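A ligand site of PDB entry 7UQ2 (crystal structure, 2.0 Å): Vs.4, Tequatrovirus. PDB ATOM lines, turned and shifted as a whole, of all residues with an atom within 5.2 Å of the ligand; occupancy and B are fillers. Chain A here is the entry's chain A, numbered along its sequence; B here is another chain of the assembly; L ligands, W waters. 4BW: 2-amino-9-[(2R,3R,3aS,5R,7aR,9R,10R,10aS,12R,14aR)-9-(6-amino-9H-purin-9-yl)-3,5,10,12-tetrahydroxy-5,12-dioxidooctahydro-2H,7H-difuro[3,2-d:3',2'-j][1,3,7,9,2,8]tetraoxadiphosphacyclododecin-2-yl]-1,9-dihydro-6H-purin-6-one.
The side-chain amino group (NZ) of Lys 10 of chain A lies close to the backbone carbonyl oxygen (O) of Gln 84 of chain A. The side-chain sulfur (SD) of Met 76 of chain B sits at hydrogen-bond distance from the guanidinium group (NH1) of Arg 80 of chain A. SD of Met 76 of chain A lies within hydrogen-bond range of NH1 of Arg 80 of chain B (3.4 Å). O of Ser 75 of chain A is in hydrogen-bond range of SG of Cys 79 of chain A. SG of Cys 79 of chain B sits at hydrogen-bond distance from O of Ser 75 of chain B (3.3 Å).
The backbone NH (N) of Lys 10 of chain A sits close to a nitrogen (NAA) of the ligand (2.6 Å). A nitrogen (NAT) of the ligand lies within hydrogen-bond range of the backbone carbonyl oxygen of Lys 10 of chain A, 2.7 Å away. OH of Tyr 9 of chain B is in hydrogen-bond range of OAD of the ligand (2.7 Å). The side-chain hydroxyl of Tyr 9 of chain A is in hydrogen-bond range of an oxygen (OAI) of the ligand (2.8 Å). NZ of Lys 24 of chain A is in salt-bridge range of OAD of the ligand (2.8 Å). OAI of the ligand lies within salt-bridge range of NZ of Lys 24 of chain B (3.0 Å). N of Lys 10 of chain B is in hydrogen-bond range of N1 of the ligand. O of Lys 10 of chain B is in hydrogen-bond range of N6 of the ligand (3.1 Å). A ring nitrogen (NE2) of His 12 of chain B is in hydrogen-bond range of a nitrogen (N6) of the ligand (3.2 Å). NE2 of His 12 of chain A lies within hydrogen-bond range of OAC of the ligand, at 3.3 Å.
Water W3 lies within hydrogen-bond range of an oxygen (OAE) of the ligand (2.5 Å), the side-chain hydroxyl of Ser 75 of chain B (2.7 Å), the side-chain amino group of Lys 24 of chain B (2.8 Å) and the side-chain sulfur of Cys 79 of chain B (3.8 Å). Water W2 lies within hydrogen-bond range of an oxygen (OAH) of the ligand, the side-chain hydroxyl of Ser 75 of chain A, the side-chain amino group of Lys 24 of chain A and the side-chain sulfur of Cys 79 of chain A. Water W4 lies within hydrogen-bond range of O2' of the ligand (3.0 Å), NZ of Lys 24 of chain A (3.2 Å) and NH2 of Arg 80 of chain B (3.4 Å). Water W1 lies within hydrogen-bond range of an oxygen (OAG) of the ligand (3.1 Å), the side-chain amino group (NZ) of Lys 24 of chain B (3.3 Å) and the guanidinium group (NH2) of Arg 80 of chain A (3.5 Å).
An oxygen (O3') of the ligand sits close to the side-chain sulfur (SD) of Met 76 of chain A (3.8 Å). An oxygen (OAZ) of the ligand sits close to the side-chain sulfur of Met 76 of chain B (3.7 Å). Merely in contact with the ligand: Ile 3 of chain A (3.9 Å), Cys 79 of chain A (3.6 Å), Arg 80 of chain A (3.5 Å), Phe 83 of chain A (3.2 Å), Gln 84 of chain A (3.9 Å), Pro 85 of chain A (3.5 Å), Ile 3 of chain B (3.8 Å), Cys 79 of chain B (3.6 Å), Arg 80 of chain B (3.5 Å), Phe 83 of chain B (3.1 Å) and Pro 85 of chain B (3.5 Å). Hydrophobic or aromatic side chains within 4 Å of the ligand: Ile 3 of chain A, Tyr 9 of chain A, His 12 of chain A, Met 76 of chain A, Phe 83 of chain A, Pro 85 of chain A, Ile 3 of chain B, Tyr 9 of chain B, His 12 of chain B, Met 76 of chain B, Phe 83 of chain B and Pro 85 of chain B. Within 4 Å of the ligand: Ile 3 of chain A, Tyr 9 of chain A, Lys 10 of chain A, His 12 of chain A, Lys 24 of chain A, Met 76 of chain A, Cys 79 of chain A, Arg 80 of chain A, Phe 83 of chain A, Gln 84 of chain A, Pro 85 of chain A, Ile 3 of chain B, Tyr 9 of chain B, Lys 10 of chain B, His 12 of chain B, Lys 24 of chain B, Met 76 of chain B, Cys 79 of chain B, Arg 80 of chain B, Phe 83 of chain B and Pro 85 of chain B.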
ATOM      1  N   ILE A   3      -9.554  15.537  20.768  1.00  0.00           N
ATOM      2  CA  ILE A   3      -9.702  15.841  19.351  1.00  0.00           C
ATOM      3  C   ILE A   3      -9.426  17.309  19.088  1.00  0.00           C
ATOM      4  O   ILE A   3      -8.956  17.684  17.997  1.00  0.00           O
ATOM      5  CB  ILE A   3     -11.103  15.435  18.856  1.00  0.00           C
ATOM      6  CG1 ILE A   3     -12.176  16.337  19.472  1.00  0.00           C
ATOM      7  CG2 ILE A   3     -11.379  13.973  19.173  1.00  0.00           C
ATOM      8  CD1 ILE A   3     -12.513  17.553  18.641  1.00  0.00           C
ATOM      9  N   GLY A   8      -8.824  21.413  12.693  1.00  0.00           N
ATOM     10  CA  GLY A   8     -10.006  21.144  11.920  1.00  0.00           C
ATOM     11  C   GLY A   8     -10.967  20.116  12.464  1.00  0.00           C
ATOM     12  O   GLY A   8     -12.051  19.954  11.948  1.00  0.00           O
ATOM     13  N   TYR A   9     -10.553  19.424  13.492  1.00  0.00           N
ATOM     14  CA  TYR A   9     -11.382  18.424  14.089  1.00  0.00           C
ATOM     15  C   TYR A   9     -12.509  19.066  14.882  1.00  0.00           C
ATOM     16  O   TYR A   9     -12.385  20.141  15.384  1.00  0.00           O
ATOM     17  CB  TYR A   9     -10.574  17.507  14.980  1.00  0.00           C
ATOM     18  CG  TYR A   9      -9.880  16.357  14.288  1.00  0.00           C
ATOM     19  CD1 TYR A   9      -9.518  16.418  12.963  1.00  0.00           C
ATOM     20  CD2 TYR A   9      -9.565  15.214  14.991  1.00  0.00           C
ATOM     21  CE1 TYR A   9      -8.888  15.350  12.351  1.00  0.00           C
ATOM     22  CE2 TYR A   9      -8.940  14.151  14.392  1.00  0.00           C
ATOM     23  CZ  TYR A   9      -8.607  14.220  13.061  1.00  0.00           C
ATOM     24  OH  TYR A   9      -7.978  13.158  12.503  1.00  0.00           O
ATOM     25  N   LYS A  10     -13.630  18.397  14.904  1.00  0.00           N
ATOM     26  CA  LYS A  10     -14.783  18.825  15.653  1.00  0.00           C
ATOM     27  C   LYS A  10     -15.193  17.701  16.574  1.00  0.00           C
ATOM     28  O   LYS A  10     -14.817  16.585  16.385  1.00  0.00           O
ATOM     29  CB  LYS A  10     -15.922  19.188  14.722  1.00  0.00           C
ATOM     30  CG  LYS A  10     -15.701  20.339  13.768  1.00  0.00           C
ATOM     31  CD  LYS A  10     -16.801  20.301  12.735  1.00  0.00           C
ATOM     32  CE  LYS A  10     -17.033  21.603  11.989  1.00  0.00           C
ATOM     33  NZ  LYS A  10     -18.099  21.496  10.925  1.00  0.00           N
ATOM     34  N   PRO A  11     -15.959  18.013  17.601  1.00  0.00           N
ATOM     35  CA  PRO A  11     -16.389  17.037  18.597  1.00  0.00           C
ATOM     36  C   PRO A  11     -17.236  15.911  18.038  1.00  0.00           C
ATOM     37  O   PRO A  11     -17.936  16.069  17.088  1.00  0.00           O
ATOM     38  CB  PRO A  11     -17.239  17.860  19.558  1.00  0.00           C
ATOM     39  CG  PRO A  11     -17.036  19.269  19.194  1.00  0.00           C
ATOM     40  CD  PRO A  11     -16.615  19.308  17.784  1.00  0.00           C
ATOM     41  N   HIS A  12     -17.137  14.774  18.694  1.00  0.00           N
ATOM     42  CA  HIS A  12     -17.897  13.624  18.343  1.00  0.00           C
ATOM     43  C   HIS A  12     -19.326  13.767  18.878  1.00  0.00           C
ATOM     44  O   HIS A  12     -19.579  14.553  19.757  1.00  0.00           O
ATOM     45  CB  HIS A  12     -17.334  12.398  19.033  1.00  0.00           C
ATOM     46  CG  HIS A  12     -15.988  11.959  18.559  1.00  0.00           C
ATOM     47  ND1 HIS A  12     -15.264  10.990  19.213  1.00  0.00           N
ATOM     48  CD2 HIS A  12     -15.238  12.331  17.511  1.00  0.00           C
ATOM     49  CE1 HIS A  12     -14.140  10.784  18.576  1.00  0.00           C
ATOM     50  NE2 HIS A  12     -14.088  11.598  17.554  1.00  0.00           N
ATOM     51  N   LYS A  24     -16.619   1.449   9.554  1.00  0.00           N
ATOM     52  CA  LYS A  24     -15.380   0.724   9.806  1.00  0.00           C
ATOM     53  C   LYS A  24     -15.643  -0.767  10.003  1.00  0.00           C
ATOM     54  O   LYS A  24     -14.843  -1.606   9.570  1.00  0.00           O
ATOM     55  CB  LYS A  24     -14.665   1.319  11.020  1.00  0.00           C
ATOM     56  CG  LYS A  24     -14.289   2.781  10.839  1.00  0.00           C
ATOM     57  CD  LYS A  24     -13.419   3.277  11.993  1.00  0.00           C
ATOM     58  CE  LYS A  24     -12.944   4.699  11.749  1.00  0.00           C
ATOM     59  NZ  LYS A  24     -11.780   4.758  10.825  1.00  0.00           N
ATOM     60  N   SER A  75     -13.154   3.992   2.943  1.00  0.00           N
ATOM     61  CA  SER A  75     -13.538   4.158   4.323  1.00  0.00           C
ATOM     62  C   SER A  75     -13.210   5.559   4.861  1.00  0.00           C
ATOM     63  O   SER A  75     -14.000   6.152   5.548  1.00  0.00           O
ATOM     64  CB  SER A  75     -12.867   3.119   5.206  1.00  0.00           C
ATOM     65  OG  SER A  75     -13.406   3.174   6.481  1.00  0.00           O
ATOM     66  N   MET A  76     -12.027   6.015   4.533  1.00  0.00           N
ATOM     67  CA  MET A  76     -11.569   7.297   4.971  1.00  0.00           C
ATOM     68  C   MET A  76     -12.456   8.415   4.435  1.00  0.00           C
ATOM     69  O   MET A  76     -12.865   9.235   5.176  1.00  0.00           O
ATOM     70  CB  MET A  76     -10.093   7.495   4.600  1.00  0.00           C
ATOM     71  CG  MET A  76      -9.152   6.721   5.502  1.00  0.00           C
ATOM     72  SD  MET A  76      -7.438   7.263   5.562  1.00  0.00           S
ATOM     73  CE  MET A  76      -6.945   7.039   3.872  1.00  0.00           C
ATOM     74  N   CYS A  79     -15.974   8.172   6.265  1.00  0.00           N
ATOM     75  CA  CYS A  79     -15.849   8.605   7.627  1.00  0.00           C
ATOM     76  C   CYS A  79     -15.692  10.141   7.699  1.00  0.00           C
ATOM     77  O   CYS A  79     -16.300  10.778   8.521  1.00  0.00           O
ATOM     78  CB  CYS A  79     -14.740   7.839   8.354  1.00  0.00           C
ATOM     79  SG  CYS A  79     -15.075   6.104   8.682  1.00  0.00           S
ATOM     80  N   ARG A  80     -14.910  10.700   6.804  1.00  0.00           N
ATOM     81  CA  ARG A  80     -14.725  12.137   6.710  1.00  0.00           C
ATOM     82  C   ARG A  80     -16.101  12.788   6.446  1.00  0.00           C
ATOM     83  O   ARG A  80     -16.422  13.775   7.023  1.00  0.00           O
ATOM     84  CB  ARG A  80     -13.758  12.530   5.617  1.00  0.00           C
ATOM     85  CG  ARG A  80     -13.349  13.988   5.602  1.00  0.00           C
ATOM     86  CD  ARG A  80     -12.494  14.326   4.393  1.00  0.00           C
ATOM     87  NE  ARG A  80     -11.998  15.685   4.384  1.00  0.00           N
ATOM     88  CZ  ARG A  80     -10.719  16.010   4.433  1.00  0.00           C
ATOM     89  NH1 ARG A  80      -9.808  15.077   4.454  1.00  0.00           N
ATOM     90  NH2 ARG A  80     -10.349  17.262   4.406  1.00  0.00           N
ATOM     91  N   PHE A  83     -17.915  12.620   9.912  1.00  0.00           N
ATOM     92  CA  PHE A  83     -17.299  13.508  10.894  1.00  0.00           C
ATOM     93  C   PHE A  83     -17.554  14.974  10.551  1.00  0.00           C
ATOM     94  O   PHE A  83     -17.863  15.779  11.436  1.00  0.00           O
ATOM     95  CB  PHE A  83     -15.795  13.238  10.968  1.00  0.00           C
ATOM     96  CG  PHE A  83     -15.417  12.074  11.837  1.00  0.00           C
ATOM     97  CD1 PHE A  83     -15.879  11.992  13.148  1.00  0.00           C
ATOM     98  CD2 PHE A  83     -14.606  11.075  11.358  1.00  0.00           C
ATOM     99  CE1 PHE A  83     -15.531  10.920  13.943  1.00  0.00           C
ATOM    100  CE2 PHE A  83     -14.250   9.998  12.157  1.00  0.00           C
ATOM    101  CZ  PHE A  83     -14.709   9.927  13.448  1.00  0.00           C
ATOM    102  N   GLN A  84     -17.400  15.331   9.279  1.00  0.00           N
ATOM    103  CA  GLN A  84     -17.583  16.705   8.807  1.00  0.00           C
ATOM    104  C   GLN A  84     -16.575  17.640   9.451  1.00  0.00           C
ATOM    105  O   GLN A  84     -16.952  18.558  10.193  1.00  0.00           O
ATOM    106  CB  GLN A  84     -19.010  17.180   9.094  1.00  0.00           C
ATOM    107  CG  GLN A  84     -20.064  16.501   8.226  1.00  0.00           C
ATOM    108  CD  GLN A  84     -21.336  17.315   8.117  1.00  0.00           C
ATOM    109  OE1 GLN A  84     -21.961  17.648   9.123  1.00  0.00           O
ATOM    110  NE2 GLN A  84     -21.735  17.630   6.889  1.00  0.00           N
ATOM    111  N   PRO A  85     -15.284  17.453   9.188  1.00  0.00           N
ATOM    112  CA  PRO A  85     -14.283  18.398   9.690  1.00  0.00           C
ATOM    113  C   PRO A  85     -14.400  19.736   8.989  1.00  0.00           C
ATOM    114  O   PRO A  85     -15.033  19.862   7.929  1.00  0.00           O
ATOM    115  CB  PRO A  85     -12.951  17.713   9.376  1.00  0.00           C
ATOM    116  CG  PRO A  85     -13.260  16.861   8.187  1.00  0.00           C
ATOM    117  CD  PRO A  85     -14.675  16.382   8.379  1.00  0.00           C
ATOM    118  N   GLU A  86     -13.773  20.741   9.586  1.00  0.00           N
ATOM    119  CA  GLU A  86     -13.643  22.019   8.894  1.00  0.00           C
ATOM    120  C   GLU A  86     -12.889  21.823   7.596  1.00  0.00           C
ATOM    121  O   GLU A  86     -11.801  21.228   7.575  1.00  0.00           O
ATOM    122  CB  GLU A  86     -12.921  23.032   9.783  1.00  0.00           C
ATOM    123  CG  GLU A  86     -12.799  24.415   9.154  1.00  0.00           C
ATOM    124  CD  GLU A  86     -12.393  25.487  10.142  1.00  0.00           C
ATOM    125  OE1 GLU A  86     -12.167  25.146  11.327  1.00  0.00           O
ATOM    126  OE2 GLU A  86     -12.301  26.669   9.744  1.00  0.00           O
ATOM    127  N   ILE B   3     -11.226   9.341  21.860  1.00  0.00           N
ATOM    128  CA  ILE B   3     -10.774   8.574  20.755  1.00  0.00           C
ATOM    129  C   ILE B   3     -11.116   7.123  20.926  1.00  0.00           C
ATOM    130  O   ILE B   3     -11.362   6.473  19.957  1.00  0.00           O
ATOM    131  CB  ILE B   3      -9.286   8.784  20.463  1.00  0.00           C
ATOM    132  CG1 ILE B   3      -8.422   8.343  21.645  1.00  0.00           C
ATOM    133  CG2 ILE B   3      -9.036  10.204  20.019  1.00  0.00           C
ATOM    134  CD1 ILE B   3      -8.015   6.901  21.600  1.00  0.00           C
ATOM    135  N   GLY B   8     -10.435   1.171  16.385  1.00  0.00           N
ATOM    136  CA  GLY B   8      -9.102   1.211  15.819  1.00  0.00           C
ATOM    137  C   GLY B   8      -8.274   2.413  16.202  1.00  0.00           C
ATOM    138  O   GLY B   8      -7.054   2.403  15.976  1.00  0.00           O
ATOM    139  N   TYR B   9      -8.888   3.460  16.764  1.00  0.00           N
ATOM    140  CA  TYR B   9      -8.133   4.638  17.149  1.00  0.00           C
ATOM    141  C   TYR B   9      -7.254   4.349  18.366  1.00  0.00           C
ATOM    142  O   TYR B   9      -7.603   3.526  19.225  1.00  0.00           O
ATOM    143  CB  TYR B   9      -9.073   5.807  17.465  1.00  0.00           C
ATOM    144  CG  TYR B   9      -9.502   6.595  16.245  1.00  0.00           C
ATOM    145  CD1 TYR B   9      -9.520   6.007  14.985  1.00  0.00           C
ATOM    146  CD2 TYR B   9      -9.909   7.914  16.368  1.00  0.00           C
ATOM    147  CE1 TYR B   9      -9.925   6.732  13.874  1.00  0.00           C
ATOM    148  CE2 TYR B   9     -10.314   8.639  15.257  1.00  0.00           C
ATOM    149  CZ  TYR B   9     -10.319   8.049  14.018  1.00  0.00           C
ATOM    150  OH  TYR B   9     -10.721   8.767  12.918  1.00  0.00           O
ATOM    151  N   LYS B  10      -6.117   5.016  18.406  1.00  0.00           N
ATOM    152  CA  LYS B  10      -5.169   4.897  19.498  1.00  0.00           C
ATOM    153  C   LYS B  10      -4.892   6.260  20.101  1.00  0.00           C
ATOM    154  O   LYS B  10      -5.079   7.253  19.464  1.00  0.00           O
ATOM    155  CB  LYS B  10      -3.907   4.179  19.056  1.00  0.00           C
ATOM    156  CG  LYS B  10      -4.189   2.768  18.585  1.00  0.00           C
ATOM    157  CD  LYS B  10      -2.966   1.895  18.504  1.00  0.00           C
ATOM    158  CE  LYS B  10      -3.362   0.459  18.746  1.00  0.00           C
ATOM    159  NZ  LYS B  10      -2.204  -0.453  18.966  1.00  0.00           N
ATOM    160  N   PRO B  11      -4.350   6.304  21.323  1.00  0.00           N
ATOM    161  CA  PRO B  11      -4.184   7.606  21.990  1.00  0.00           C
ATOM    162  C   PRO B  11      -3.225   8.512  21.225  1.00  0.00           C
ATOM    163  O   PRO B  11      -2.292   8.051  20.566  1.00  0.00           O
ATOM    164  CB  PRO B  11      -3.619   7.238  23.367  1.00  0.00           C
ATOM    165  CG  PRO B  11      -3.970   5.789  23.558  1.00  0.00           C
ATOM    166  CD  PRO B  11      -3.936   5.184  22.185  1.00  0.00           C
ATOM    167  N   HIS B  12      -3.467   9.808  21.339  1.00  0.00           N
ATOM    168  CA  HIS B  12      -2.539  10.786  20.790  1.00  0.00           C
ATOM    169  C   HIS B  12      -1.259  10.816  21.610  1.00  0.00           C
ATOM    170  O   HIS B  12      -1.187  10.306  22.732  1.00  0.00           O
ATOM    171  CB  HIS B  12      -3.157  12.189  20.785  1.00  0.00           C
ATOM    172  CG  HIS B  12      -4.370  12.325  19.914  1.00  0.00           C
ATOM    173  ND1 HIS B  12      -5.102  13.484  19.842  1.00  0.00           N
ATOM    174  CD2 HIS B  12      -4.977  11.444  19.084  1.00  0.00           C
ATOM    175  CE1 HIS B  12      -6.107  13.313  19.002  1.00  0.00           C
ATOM    176  NE2 HIS B  12      -6.053  12.083  18.535  1.00  0.00           N
ATOM    177  N   LYS B  24      -1.118  18.969   8.104  1.00  0.00           N
ATOM    178  CA  LYS B  24      -2.338  19.684   7.757  1.00  0.00           C
ATOM    179  C   LYS B  24      -2.056  21.150   7.433  1.00  0.00           C
ATOM    180  O   LYS B  24      -2.673  21.713   6.517  1.00  0.00           O
ATOM    181  CB  LYS B  24      -3.348  19.563   8.895  1.00  0.00           C
ATOM    182  CG  LYS B  24      -3.902  18.149   9.086  1.00  0.00           C
ATOM    183  CD  LYS B  24      -4.840  18.057  10.274  1.00  0.00           C
ATOM    184  CE  LYS B  24      -5.350  16.635  10.466  1.00  0.00           C
ATOM    185  NZ  LYS B  24      -6.248  16.193   9.368  1.00  0.00           N
ATOM    186  N   SER B  75      -2.930  14.023   2.315  1.00  0.00           N
ATOM    187  CA  SER B  75      -2.906  14.367   3.723  1.00  0.00           C
ATOM    188  C   SER B  75      -3.481  13.260   4.625  1.00  0.00           C
ATOM    189  O   SER B  75      -2.942  12.973   5.654  1.00  0.00           O
ATOM    190  CB  SER B  75      -3.619  15.686   3.966  1.00  0.00           C
ATOM    191  OG  SER B  75      -3.503  16.067   5.299  1.00  0.00           O
ATOM    192  N   MET B  76      -4.552  12.668   4.197  1.00  0.00           N
ATOM    193  CA  MET B  76      -5.156  11.623   4.975  1.00  0.00           C
ATOM    194  C   MET B  76      -4.184  10.428   5.138  1.00  0.00           C
ATOM    195  O   MET B  76      -4.034   9.906   6.193  1.00  0.00           O
ATOM    196  CB  MET B  76      -6.519  11.217   4.405  1.00  0.00           C
ATOM    197  CG  MET B  76      -7.634  12.213   4.692  1.00  0.00           C
ATOM    198  SD  MET B  76      -9.342  11.730   4.415  1.00  0.00           S
ATOM    199  CE  MET B  76      -9.329  11.507   2.668  1.00  0.00           C
ATOM    200  N   CYS B  79      -1.280  11.564   7.464  1.00  0.00           N
ATOM    201  CA  CYS B  79      -1.757  11.641   8.805  1.00  0.00           C
ATOM    202  C   CYS B  79      -1.993  10.247   9.386  1.00  0.00           C
ATOM    203  O   CYS B  79      -1.688   9.998  10.524  1.00  0.00           O
ATOM    204  CB  CYS B  79      -2.988  12.526   8.912  1.00  0.00           C
ATOM    205  SG  CYS B  79      -2.636  14.268   8.650  1.00  0.00           S
ATOM    206  N   ARG B  80      -2.496   9.341   8.568  1.00  0.00           N
ATOM    207  CA  ARG B  80      -2.746   7.962   8.978  1.00  0.00           C
ATOM    208  C   ARG B  80      -1.433   7.311   9.366  1.00  0.00           C
ATOM    209  O   ARG B  80      -1.355   6.665  10.356  1.00  0.00           O
ATOM    210  CB  ARG B  80      -3.395   7.140   7.884  1.00  0.00           C
ATOM    211  CG  ARG B  80      -3.774   5.731   8.305  1.00  0.00           C
ATOM    212  CD  ARG B  80      -4.489   4.987   7.196  1.00  0.00           C
ATOM    213  NE  ARG B  80      -4.995   3.696   7.590  1.00  0.00           N
ATOM    214  CZ  ARG B  80      -6.261   3.339   7.511  1.00  0.00           C
ATOM    215  NH1 ARG B  80      -7.145   4.159   7.033  1.00  0.00           N
ATOM    216  NH2 ARG B  80      -6.622   2.150   7.882  1.00  0.00           N
ATOM    217  N   PHE B  83      -0.474   8.809  12.900  1.00  0.00           N
ATOM    218  CA  PHE B  83      -1.336   8.337  13.956  1.00  0.00           C
ATOM    219  C   PHE B  83      -1.132   6.859  14.296  1.00  0.00           C
ATOM    220  O   PHE B  83      -1.197   6.491  15.432  1.00  0.00           O
ATOM    221  CB  PHE B  83      -2.791   8.540  13.589  1.00  0.00           C
ATOM    222  CG  PHE B  83      -3.298   9.912  13.858  1.00  0.00           C
ATOM    223  CD1 PHE B  83      -3.217  10.454  15.118  1.00  0.00           C
ATOM    224  CD2 PHE B  83      -3.874  10.645  12.849  1.00  0.00           C
ATOM    225  CE1 PHE B  83      -3.689  11.716  15.365  1.00  0.00           C
ATOM    226  CE2 PHE B  83      -4.355  11.911  13.092  1.00  0.00           C
ATOM    227  CZ  PHE B  83      -4.258  12.437  14.356  1.00  0.00           C
ATOM    228  N   GLN B  84      -0.911   6.069  13.264  1.00  0.00           N
ATOM    229  CA  GLN B  84      -0.726   4.662  13.374  1.00  0.00           C
ATOM    230  C   GLN B  84      -1.866   3.988  14.108  1.00  0.00           C
ATOM    231  O   GLN B  84      -1.704   3.410  15.135  1.00  0.00           O
ATOM    232  CB  GLN B  84       0.621   4.278  14.002  1.00  0.00           C
ATOM    233  CG  GLN B  84       1.832   4.654  13.219  1.00  0.00           C
ATOM    234  CD  GLN B  84       3.077   4.018  13.773  1.00  0.00           C
ATOM    235  OE1 GLN B  84       3.241   3.915  14.962  1.00  0.00           O
ATOM    236  NE2 GLN B  84       3.932   3.555  12.889  1.00  0.00           N
ATOM    237  N   PRO B  85      -3.057   4.006  13.488  1.00  0.00           N
ATOM    238  CA  PRO B  85      -4.185   3.290  14.044  1.00  0.00           C
ATOM    239  C   PRO B  85      -4.014   1.788  13.909  1.00  0.00           C
ATOM    240  O   PRO B  85      -3.199   1.274  13.196  1.00  0.00           O
ATOM    241  CB  PRO B  85      -5.332   3.688  13.136  1.00  0.00           C
ATOM    242  CG  PRO B  85      -4.711   4.102  11.883  1.00  0.00           C
ATOM    243  CD  PRO B  85      -3.387   4.688  12.242  1.00  0.00           C
HETATM  244  OAC 4BW L   1     -12.841  13.951  15.591  1.00  0.00           O
HETATM  245  CBC 4BW L   1     -12.986  14.277  14.471  1.00  0.00           C
HETATM  246  NAT 4BW L   1     -13.729  15.396  14.244  1.00  0.00           N
HETATM  247  CBA 4BW L   1     -13.960  15.860  12.965  1.00  0.00           C
HETATM  248  NAA 4BW L   1     -14.777  17.056  13.043  1.00  0.00           N
HETATM  249  NAS 4BW L   1     -13.441  15.205  11.760  1.00  0.00           N
HETATM  250  CBG 4BW L   1     -12.651  13.974  11.986  1.00  0.00           C
HETATM  251  CBE 4BW L   1     -12.421  13.504  13.236  1.00  0.00           C
HETATM  252  NAR 4BW L   1     -11.692  12.413  13.140  1.00  0.00           N
HETATM  253  CAL 4BW L   1     -11.473  12.187  11.838  1.00  0.00           C
HETATM  254  NBQ 4BW L   1     -12.058  13.161  11.131  1.00  0.00           N
HETATM  255  CBO 4BW L   1     -11.999  13.184   9.677  1.00  0.00           C
HETATM  256  CBI 4BW L   1     -10.574  13.629   9.270  1.00  0.00           C
HETATM  257  OAG 4BW L   1     -10.664  14.480   8.227  1.00  0.00           O
HETATM  258  OAX 4BW L   1     -12.209  12.014   9.164  1.00  0.00           O
HETATM  259  CBK 4BW L   1     -10.967  11.671   8.294  1.00  0.00           C
HETATM  260  CAN 4BW L   1     -10.741  10.168   8.146  1.00  0.00           C
HETATM  261  OAV 4BW L   1     -10.851   9.468   9.356  1.00  0.00           O
HETATM  262  PBR 4BW L   1     -10.501   7.921   9.330  1.00  0.00           P
HETATM  263  O3' 4BW L   1      -8.924   7.948   8.985  1.00  0.00           O
HETATM  264  OAH 4BW L   1     -11.229   7.220   8.400  1.00  0.00           O
HETATM  265  OAD 4BW L   1     -10.707   7.345  10.577  1.00  0.00           O
HETATM  266  CBM 4BW L   1      -9.968  12.305   8.923  1.00  0.00           C
HETATM  267  OAZ 4BW L   1      -8.776  12.508   8.001  1.00  0.00           O
HETATM  268  PBS 4BW L   1      -7.306  12.640   8.636  1.00  0.00           P
HETATM  269  OAI 4BW L   1      -7.386  13.404   9.796  1.00  0.00           O
HETATM  270  OAE 4BW L   1      -6.389  13.173   7.787  1.00  0.00           O
HETATM  271  O5' 4BW L   1      -6.645  11.180   9.049  1.00  0.00           O
HETATM  272  C5' 4BW L   1      -7.501  10.374   9.658  1.00  0.00           C
HETATM  273  C4' 4BW L   1      -6.989   8.956   9.620  1.00  0.00           C
HETATM  274  O4' 4BW L   1      -5.759   8.721  10.604  1.00  0.00           O
HETATM  275  C3' 4BW L   1      -8.029   8.330  10.108  1.00  0.00           C
HETATM  276  C2' 4BW L   1      -7.456   7.208  10.965  1.00  0.00           C
HETATM  277  O2' 4BW L   1      -7.196   6.103  10.308  1.00  0.00           O
HETATM  278  C1' 4BW L   1      -6.162   7.907  11.506  1.00  0.00           C
HETATM  279  N9  4BW L   1      -6.534   8.657  12.700  1.00  0.00           N
HETATM  280  C8  4BW L   1      -7.198   9.754  12.910  1.00  0.00           C
HETATM  281  N7  4BW L   1      -7.225   9.907  14.201  1.00  0.00           N
HETATM  282  C5  4BW L   1      -6.569   8.897  14.762  1.00  0.00           C
HETATM  283  C4  4BW L   1      -6.123   8.087  13.842  1.00  0.00           C
HETATM  284  N3  4BW L   1      -5.438   6.980  14.214  1.00  0.00           N
HETATM  285  C2  4BW L   1      -5.200   6.720  15.520  1.00  0.00           C
HETATM  286  N1  4BW L   1      -5.664   7.576  16.445  1.00  0.00           N
HETATM  287  C6  4BW L   1      -6.319   8.635  16.088  1.00  0.00           C
HETATM  288  N6  4BW L   1      -6.541   9.093  17.369  1.00  0.00           N
HETATM  289  O   HOH W   1      -8.825  16.855   7.488  1.00  0.00           O
HETATM  290  O   HOH W   2     -11.716   4.715   8.035  1.00  0.00           O
HETATM  291  O   HOH W   3      -5.699  15.305   6.724  1.00  0.00           O
HETATM  292  O   HOH W   4      -8.826   3.653  10.061  1.00  0.00           O
HETATM  293  O   HOH W   5      -2.646   7.903  17.577  1.00  0.00           O
HETATM  294  O   HOH W   6     -16.937  15.207  14.398  1.00  0.00           O
